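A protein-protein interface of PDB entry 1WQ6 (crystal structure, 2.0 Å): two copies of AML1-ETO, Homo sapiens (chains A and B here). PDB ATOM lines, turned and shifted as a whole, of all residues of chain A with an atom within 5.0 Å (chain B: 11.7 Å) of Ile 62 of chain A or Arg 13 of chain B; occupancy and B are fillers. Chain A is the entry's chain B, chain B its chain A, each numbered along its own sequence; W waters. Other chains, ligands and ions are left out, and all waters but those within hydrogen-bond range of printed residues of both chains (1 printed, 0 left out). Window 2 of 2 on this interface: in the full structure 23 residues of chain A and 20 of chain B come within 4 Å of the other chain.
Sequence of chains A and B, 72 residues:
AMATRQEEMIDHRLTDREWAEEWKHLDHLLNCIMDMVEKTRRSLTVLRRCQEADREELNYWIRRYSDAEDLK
The guanidinium group (NH2) of Arg 13 of chain B is in hydrogen-bond range of the side-chain amide oxygen (OD1) of Asn 59 of chain A (3.2 Å).
NH2 of Arg 55 of chain A sits at hydrogen-bond distance from O of Leu 14 of chain B, 2.5 Å away.
NH1 of Arg 55 of chain A sits close to NE of Arg 13 of chain B, at 2.9 Å.
The indole nitrogen (NE1) of Trp 19 of chain B sits close to the guanidinium group (NH2) of Arg 55 of chain A (3.0 Å).
Among the printed residues, pairs that only touch across the chains: Arg 55 of chain A with Asp 16 of chain B, Leu 58 of chain A with Arg 13 of chain B and Ile 62 of chain A with Arg 13 of chain B.
Printed residues of chain B within 4 Å of Arg 55 of chain A: Arg 13 (2.9 Å), Leu 14 (2.5 Å), Asp 16 (3.7 Å) and Trp 19 (3.0 Å).
Leu 58 of chain A touches just one residue of chain B: Arg 13.
Asn 59 of chain A touches just one residue of chain B: Arg 13 (3.2 Å).
Tyr 60 of chain A touches none of the printed residues of chain B.
Arg 64 of chain A touches none of the printed residues of chain B.
No residue of chain B comes within 4 Å of Ser 66 of chain A.
Of the printed residues of chain A, Arg 13 of chain B touches Arg 55 (2.9 Å), Leu 58 (3.7 Å), Asn 59 (3.2 Å) and Ile 62 (3.6 Å).
Of the printed residues of chain A, Leu 14 of chain B touches Arg 55.
Of the printed residues of chain A, Asp 16 of chain B touches Arg 55 (3.7 Å).
Of the printed residues of chain A, Trp 19 of chain B touches Arg 55 (3.0 Å).
The nearest residue of chain B that does not touch Ile 62 of chain A is Asp 11 of chain B (8.6 Å).
The nearest printed residue of chain A that does not touch Trp 19 of chain B is Leu 58 of chain A (7.4 Å).
Hydrophobic or aromatic side chains of chain A within 4 Å of the printed part of chain B: Leu 58 and Ile 62.
Among the printed residues, 7 pairs touch across the chains.
Among the printed residues, no Asp or Glu carboxylate lies within 4 Å of a Lys or Arg side-chain nitrogen of the other chain.
No position is printed for both chains.
Water W1 lies within hydrogen-bond range of OD1 of Asp 16 of chain B (2.6 Å) and ND2 of Asn 59 of chain A (2.8 Å).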
ATOM      1  N   ARG A  55      20.059   5.712  32.480  1.00  0.00           N
ATOM      2  CA  ARG A  55      19.748   5.503  31.048  1.00  0.00           C
ATOM      3  C   ARG A  55      18.240   5.210  30.910  1.00  0.00           C
ATOM      4  O   ARG A  55      17.655   5.731  29.988  1.00  0.00           O
ATOM      5  CB  ARG A  55      20.539   4.290  30.501  1.00  0.00           C
ATOM      6  CG  ARG A  55      20.245   3.940  29.025  1.00  0.00           C
ATOM      7  CD  ARG A  55      20.456   5.178  28.118  1.00  0.00           C
ATOM      8  NE  ARG A  55      21.759   4.940  27.517  1.00  0.00           N
ATOM      9  CZ  ARG A  55      22.437   5.912  27.077  1.00  0.00           C
ATOM     10  NH1 ARG A  55      21.895   7.103  27.201  1.00  0.00           N
ATOM     11  NH2 ARG A  55      23.617   5.761  26.605  1.00  0.00           N
ATOM     12  N   LEU A  58      16.610   8.579  31.392  1.00  0.00           N
ATOM     13  CA  LEU A  58      16.837   9.322  30.152  1.00  0.00           C
ATOM     14  C   LEU A  58      15.895   8.896  29.003  1.00  0.00           C
ATOM     15  O   LEU A  58      15.254   9.764  28.375  1.00  0.00           O
ATOM     16  CB  LEU A  58      18.326   9.270  29.790  1.00  0.00           C
ATOM     17  CG  LEU A  58      18.788   9.786  28.423  1.00  0.00           C
ATOM     18  CD1 LEU A  58      18.552  11.247  28.164  1.00  0.00           C
ATOM     19  CD2 LEU A  58      20.291   9.451  28.245  1.00  0.00           C
ATOM     20  N   ASN A  59      15.806   7.588  28.710  1.00  0.00           N
ATOM     21  CA  ASN A  59      14.969   7.158  27.645  1.00  0.00           C
ATOM     22  C   ASN A  59      13.490   7.470  27.932  1.00  0.00           C
ATOM     23  O   ASN A  59      12.785   7.798  27.016  1.00  0.00           O
ATOM     24  CB  ASN A  59      15.106   5.646  27.354  1.00  0.00           C
ATOM     25  CG  ASN A  59      16.473   5.277  26.808  1.00  0.00           C
ATOM     26  OD1 ASN A  59      17.131   6.119  26.176  1.00  0.00           O
ATOM     27  ND2 ASN A  59      16.847   3.995  26.977  1.00  0.00           N
ATOM     28  N   TYR A  60      13.095   7.441  29.193  1.00  0.00           N
ATOM     29  CA  TYR A  60      11.748   7.743  29.615  1.00  0.00           C
ATOM     30  C   TYR A  60      11.433   9.204  29.328  1.00  0.00           C
ATOM     31  O   TYR A  60      10.437   9.552  28.654  1.00  0.00           O
ATOM     32  CB  TYR A  60      11.642   7.610  31.104  1.00  0.00           C
ATOM     33  CG  TYR A  60      10.258   7.983  31.486  1.00  0.00           C
ATOM     34  CD1 TYR A  60       9.173   7.178  31.013  1.00  0.00           C
ATOM     35  CD2 TYR A  60      10.014   9.100  32.287  1.00  0.00           C
ATOM     36  CE1 TYR A  60       7.901   7.483  31.353  1.00  0.00           C
ATOM     37  CE2 TYR A  60       8.703   9.423  32.661  1.00  0.00           C
ATOM     38  CZ  TYR A  60       7.661   8.580  32.178  1.00  0.00           C
ATOM     39  OH  TYR A  60       6.332   8.788  32.420  1.00  0.00           O
ATOM     40  N   TRP A  61      12.323  10.095  29.780  1.00  0.00           N
ATOM     41  CA  TRP A  61      12.173  11.522  29.430  1.00  0.00           C
ATOM     42  C   TRP A  61      12.258  11.930  27.968  1.00  0.00           C
ATOM     43  O   TRP A  61      11.530  12.808  27.464  1.00  0.00           O
ATOM     44  CB  TRP A  61      12.974  12.436  30.372  1.00  0.00           C
ATOM     45  CG  TRP A  61      12.439  12.413  31.727  1.00  0.00           C
ATOM     46  CD1 TRP A  61      12.926  11.745  32.814  1.00  0.00           C
ATOM     47  CD2 TRP A  61      11.187  13.010  32.139  1.00  0.00           C
ATOM     48  NE1 TRP A  61      12.108  11.989  33.887  1.00  0.00           N
ATOM     49  CE2 TRP A  61      11.023  12.727  33.500  1.00  0.00           C
ATOM     50  CE3 TRP A  61      10.212  13.747  31.472  1.00  0.00           C
ATOM     51  CZ2 TRP A  61       9.918  13.171  34.239  1.00  0.00           C
ATOM     52  CZ3 TRP A  61       9.093  14.166  32.195  1.00  0.00           C
ATOM     53  CH2 TRP A  61       8.970  13.901  33.566  1.00  0.00           C
ATOM     54  N   ILE A  62      13.079  11.255  27.185  1.00  0.00           N
ATOM     55  CA  ILE A  62      13.066  11.522  25.760  1.00  0.00           C
ATOM     56  C   ILE A  62      11.682  11.197  25.189  1.00  0.00           C
ATOM     57  O   ILE A  62      11.133  11.969  24.389  1.00  0.00           O
ATOM     58  CB  ILE A  62      14.174  10.688  25.078  1.00  0.00           C
ATOM     59  CG1 ILE A  62      15.555  11.233  25.499  1.00  0.00           C
ATOM     60  CG2 ILE A  62      14.201  10.748  23.545  1.00  0.00           C
ATOM     61  CD1 ILE A  62      16.727  10.331  25.084  1.00  0.00           C
ATOM     62  N   ARG A  63      11.225   9.982  25.471  1.00  0.00           N
ATOM     63  CA  ARG A  63       9.880   9.560  25.146  1.00  0.00           C
ATOM     64  C   ARG A  63       8.798  10.534  25.597  1.00  0.00           C
ATOM     65  O   ARG A  63       8.035  10.897  24.734  1.00  0.00           O
ATOM     66  CB  ARG A  63       9.669   8.142  25.680  1.00  0.00           C
ATOM     67  CG  ARG A  63       8.236   7.582  25.469  1.00  0.00           C
ATOM     68  CD  ARG A  63       7.935   7.305  24.012  1.00  0.00           C
ATOM     69  NE  ARG A  63       6.593   6.761  23.877  1.00  0.00           N
ATOM     70  CZ  ARG A  63       6.241   5.455  24.055  1.00  0.00           C
ATOM     71  NH1 ARG A  63       7.136   4.500  24.326  1.00  0.00           N
ATOM     72  NH2 ARG A  63       4.951   5.105  23.961  1.00  0.00           N
ATOM     73  N   ARG A  64       8.725  10.957  26.876  1.00  0.00           N
ATOM     74  CA  ARG A  64       7.909  12.068  27.323  1.00  0.00           C
ATOM     75  C   ARG A  64       7.970  13.296  26.431  1.00  0.00           C
ATOM     76  O   ARG A  64       6.956  13.736  25.832  1.00  0.00           O
ATOM     77  CB  ARG A  64       8.182  12.332  28.784  1.00  0.00           C
ATOM     78  CG  ARG A  64       7.401  11.339  29.652  1.00  0.00           C
ATOM     79  CD  ARG A  64       5.954  11.843  29.905  1.00  0.00           C
ATOM     80  NE  ARG A  64       5.812  11.823  31.347  1.00  0.00           N
ATOM     81  CZ  ARG A  64       5.116  12.639  32.065  1.00  0.00           C
ATOM     82  NH1 ARG A  64       4.425  13.591  31.469  1.00  0.00           N
ATOM     83  NH2 ARG A  64       5.159  12.485  33.386  1.00  0.00           N
ATOM     84  N   TYR A  65       9.151  13.866  26.220  1.00  0.00           N
ATOM     85  CA  TYR A  65       9.217  15.009  25.375  1.00  0.00           C
ATOM     86  C   TYR A  65       8.654  14.806  23.955  1.00  0.00           C
ATOM     87  O   TYR A  65       7.887  15.615  23.396  1.00  0.00           O
ATOM     88  CB  TYR A  65      10.677  15.588  25.352  1.00  0.00           C
ATOM     89  CG  TYR A  65      10.669  16.938  24.663  1.00  0.00           C
ATOM     90  CD1 TYR A  65      10.373  18.065  25.360  1.00  0.00           C
ATOM     91  CD2 TYR A  65      10.828  17.055  23.313  1.00  0.00           C
ATOM     92  CE1 TYR A  65      10.305  19.302  24.788  1.00  0.00           C
ATOM     93  CE2 TYR A  65      10.747  18.325  22.710  1.00  0.00           C
ATOM     94  CZ  TYR A  65      10.467  19.432  23.508  1.00  0.00           C
ATOM     95  OH  TYR A  65      10.346  20.698  23.075  1.00  0.00           O
ATOM     96  N   SER A  66       9.051  13.735  23.313  1.00  0.00           N
ATOM     97  CA  SER A  66       8.551  13.418  22.013  1.00  0.00           C
ATOM     98  C   SER A  66       7.035  13.169  21.958  1.00  0.00           C
ATOM     99  O   SER A  66       6.440  13.601  20.955  1.00  0.00           O
ATOM    100  CB  SER A  66       9.301  12.244  21.402  1.00  0.00           C
ATOM    101  OG  SER A  66       8.373  11.581  20.564  1.00  0.00           O
ATOM    102  N   ASP A  67       6.434  12.619  23.022  1.00  0.00           N
ATOM    103  CA  ASP A  67       4.989  12.391  23.089  1.00  0.00           C
ATOM    104  C   ASP A  67       4.329  13.782  23.198  1.00  0.00           C
ATOM    105  O   ASP A  67       3.306  13.979  22.567  1.00  0.00           O
ATOM    106  CB  ASP A  67       4.602  11.409  24.187  1.00  0.00           C
ATOM    107  CG  ASP A  67       4.827   9.949  23.764  1.00  0.00           C
ATOM    108  OD1 ASP A  67       4.936   9.616  22.554  1.00  0.00           O
ATOM    109  OD2 ASP A  67       4.869   9.024  24.573  1.00  0.00           O
ATOM    110  N   ASP B  11      23.943  10.858  20.348  1.00  0.00           N
ATOM    111  CA  ASP B  11      24.467  10.182  19.120  1.00  0.00           C
ATOM    112  C   ASP B  11      25.959   9.864  19.298  1.00  0.00           C
ATOM    113  O   ASP B  11      26.489   8.930  18.677  1.00  0.00           O
ATOM    114  CB  ASP B  11      24.156  11.003  17.849  1.00  0.00           C
ATOM    115  CG  ASP B  11      25.358  11.777  17.309  1.00  0.00           C
ATOM    116  OD1 ASP B  11      25.527  12.940  17.740  1.00  0.00           O
ATOM    117  OD2 ASP B  11      26.167  11.330  16.451  1.00  0.00           O
ATOM    118  N   HIS B  12      26.630  10.635  20.155  1.00  0.00           N
ATOM    119  CA  HIS B  12      27.932  10.208  20.673  1.00  0.00           C
ATOM    120  C   HIS B  12      27.789   9.442  21.994  1.00  0.00           C
ATOM    121  O   HIS B  12      28.787   8.933  22.503  1.00  0.00           O
ATOM    122  CB  HIS B  12      28.973  11.353  20.650  1.00  0.00           C
ATOM    123  CG  HIS B  12      29.397  11.682  19.246  1.00  0.00           C
ATOM    124  ND1 HIS B  12      28.592  12.402  18.380  1.00  0.00           N
ATOM    125  CD2 HIS B  12      30.481  11.298  18.527  1.00  0.00           C
ATOM    126  CE1 HIS B  12      29.183  12.480  17.199  1.00  0.00           C
ATOM    127  NE2 HIS B  12      30.330  11.822  17.263  1.00  0.00           N
ATOM    128  N   ARG B  13      26.563   9.319  22.513  1.00  0.00           N
ATOM    129  CA  ARG B  13      26.307   8.451  23.660  1.00  0.00           C
ATOM    130  C   ARG B  13      26.074   7.004  23.250  1.00  0.00           C
ATOM    131  O   ARG B  13      25.439   6.705  22.226  1.00  0.00           O
ATOM    132  CB  ARG B  13      25.107   8.915  24.465  1.00  0.00           C
ATOM    133  CG  ARG B  13      23.776   8.825  23.764  1.00  0.00           C
ATOM    134  CD  ARG B  13      22.694   9.606  24.542  1.00  0.00           C
ATOM    135  NE  ARG B  13      21.586   8.704  24.855  1.00  0.00           N
ATOM    136  CZ  ARG B  13      20.330   8.795  24.426  1.00  0.00           C
ATOM    137  NH1 ARG B  13      19.925   9.770  23.607  1.00  0.00           N
ATOM    138  NH2 ARG B  13      19.477   7.841  24.812  1.00  0.00           N
ATOM    139  N   LEU B  14      26.494   6.100  24.123  1.00  0.00           N
ATOM    140  CA  LEU B  14      26.484   4.671  23.808  1.00  0.00           C
ATOM    141  C   LEU B  14      25.114   3.991  23.830  1.00  0.00           C
ATOM    142  O   LEU B  14      24.218   4.403  24.588  1.00  0.00           O
ATOM    143  CB  LEU B  14      27.438   3.998  24.802  1.00  0.00           C
ATOM    144  CG  LEU B  14      28.688   4.782  25.158  1.00  0.00           C
ATOM    145  CD1 LEU B  14      29.406   4.076  26.333  1.00  0.00           C
ATOM    146  CD2 LEU B  14      29.545   4.764  23.903  1.00  0.00           C
ATOM    147  N   THR B  15      24.912   2.980  22.985  1.00  0.00           N
ATOM    148  CA  THR B  15      23.770   2.100  23.071  1.00  0.00           C
ATOM    149  C   THR B  15      23.816   1.277  24.352  1.00  0.00           C
ATOM    150  O   THR B  15      24.816   1.209  25.050  1.00  0.00           O
ATOM    151  CB  THR B  15      23.671   1.125  21.855  1.00  0.00           C
ATOM    152  OG1 THR B  15      24.796   0.241  21.842  1.00  0.00           O
ATOM    153  CG2 THR B  15      23.624   1.882  20.498  1.00  0.00           C
ATOM    154  N   ASP B  16      22.750   0.559  24.607  1.00  0.00           N
ATOM    155  CA  ASP B  16      22.734  -0.349  25.744  1.00  0.00           C
ATOM    156  C   ASP B  16      23.842  -1.371  25.645  1.00  0.00           C
ATOM    157  O   ASP B  16      24.566  -1.726  26.604  1.00  0.00           O
ATOM    158  CB  ASP B  16      21.415  -1.092  25.908  1.00  0.00           C
ATOM    159  CG  ASP B  16      20.284  -0.183  26.451  1.00  0.00           C
ATOM    160  OD1 ASP B  16      20.584   0.925  26.977  1.00  0.00           O
ATOM    161  OD2 ASP B  16      19.078  -0.570  26.385  1.00  0.00           O
ATOM    162  N   ARG B  17      23.932  -1.987  24.469  1.00  0.00           N
ATOM    163  CA  ARG B  17      25.012  -2.928  24.208  1.00  0.00           C
ATOM    164  C   ARG B  17      26.416  -2.344  24.323  1.00  0.00           C
ATOM    165  O   ARG B  17      27.282  -3.028  24.907  1.00  0.00           O
ATOM    166  CB  ARG B  17      24.794  -3.621  22.808  1.00  0.00           C
ATOM    167  CG  ARG B  17      25.787  -4.753  22.703  1.00  0.00           C
ATOM    168  CD  ARG B  17      25.467  -5.639  21.462  1.00  0.00           C
ATOM    169  NE  ARG B  17      25.732  -4.834  20.260  1.00  0.00           N
ATOM    170  CZ  ARG B  17      25.386  -5.264  19.044  1.00  0.00           C
ATOM    171  NH1 ARG B  17      24.696  -6.381  18.924  1.00  0.00           N
ATOM    172  NH2 ARG B  17      25.632  -4.565  17.949  1.00  0.00           N
ATOM    173  N   GLU B  18      26.693  -1.158  23.783  1.00  0.00           N
ATOM    174  CA  GLU B  18      27.973  -0.538  23.991  1.00  0.00           C
ATOM    175  C   GLU B  18      28.343  -0.325  25.482  1.00  0.00           C
ATOM    176  O   GLU B  18      29.492  -0.530  25.879  1.00  0.00           O
ATOM    177  CB  GLU B  18      27.997   0.793  23.309  1.00  0.00           C
ATOM    178  CG  GLU B  18      27.987   0.558  21.763  1.00  0.00           C
ATOM    179  CD  GLU B  18      27.847   1.855  20.948  1.00  0.00           C
ATOM    180  OE1 GLU B  18      27.468   2.925  21.507  1.00  0.00           O
ATOM    181  OE2 GLU B  18      28.097   1.838  19.721  1.00  0.00           O
ATOM    182  N   TRP B  19      27.344   0.024  26.302  1.00  0.00           N
ATOM    183  CA  TRP B  19      27.596   0.248  27.742  1.00  0.00           C
ATOM    184  C   TRP B  19      27.933  -1.109  28.369  1.00  0.00           C
ATOM    185  O   TRP B  19      28.959  -1.237  29.078  1.00  0.00           O
ATOM    186  CB  TRP B  19      26.338   0.828  28.379  1.00  0.00           C
ATOM    187  CG  TRP B  19      26.307   2.268  28.485  1.00  0.00           C
ATOM    188  CD1 TRP B  19      25.390   3.113  27.990  1.00  0.00           C
ATOM    189  CD2 TRP B  19      27.216   3.055  29.224  1.00  0.00           C
ATOM    190  NE1 TRP B  19      25.745   4.413  28.265  1.00  0.00           N
ATOM    191  CE2 TRP B  19      26.819   4.397  29.094  1.00  0.00           C
ATOM    192  CE3 TRP B  19      28.346   2.774  29.979  1.00  0.00           C
ATOM    193  CZ2 TRP B  19      27.478   5.443  29.737  1.00  0.00           C
ATOM    194  CZ3 TRP B  19      28.973   3.791  30.618  1.00  0.00           C
ATOM    195  CH2 TRP B  19      28.567   5.100  30.466  1.00  0.00           C
ATOM    196  N   ALA B  20      27.150  -2.141  28.029  1.00  0.00           N
ATOM    197  CA  ALA B  20      27.393  -3.483  28.507  1.00  0.00           C
ATOM    198  C   ALA B  20      28.785  -3.991  28.155  1.00  0.00           C
ATOM    199  O   ALA B  20      29.474  -4.562  28.990  1.00  0.00           O
ATOM    200  CB  ALA B  20      26.278  -4.446  28.163  1.00  0.00           C
ATOM    201  N   GLU B  21      29.251  -3.756  26.932  1.00  0.00           N
ATOM    202  CA  GLU B  21      30.628  -4.031  26.584  1.00  0.00           C
ATOM    203  C   GLU B  21      31.690  -3.310  27.417  1.00  0.00           C
ATOM    204  O   GLU B  21      32.739  -3.825  27.809  1.00  0.00           O
ATOM    205  CB  GLU B  21      30.841  -3.667  25.103  1.00  0.00           C
ATOM    206  CG  GLU B  21      30.136  -4.689  24.250  1.00  0.00           C
ATOM    207  CD  GLU B  21      29.716  -4.420  22.774  1.00  0.00           C
ATOM    208  OE1 GLU B  21      29.445  -3.331  22.184  1.00  0.00           O
ATOM    209  OE2 GLU B  21      29.565  -5.503  22.140  1.00  0.00           O
ATOM    210  N   GLU B  22      31.491  -2.039  27.593  1.00  0.00           N
ATOM    211  CA  GLU B  22      32.375  -1.285  28.417  1.00  0.00           C
ATOM    212  C   GLU B  22      32.536  -1.908  29.803  1.00  0.00           C
ATOM    213  O   GLU B  22      33.649  -2.056  30.313  1.00  0.00           O
ATOM    214  CB  GLU B  22      31.827   0.110  28.658  1.00  0.00           C
ATOM    215  CG  GLU B  22      31.998   1.141  27.576  1.00  0.00           C
ATOM    216  CD  GLU B  22      33.411   1.227  27.074  1.00  0.00           C
ATOM    217  OE1 GLU B  22      34.355   0.830  27.811  1.00  0.00           O
ATOM    218  OE2 GLU B  22      33.510   1.725  25.929  1.00  0.00           O
HETATM  219  O   HOH W   1      19.161   2.792  25.849  1.00  0.00           O
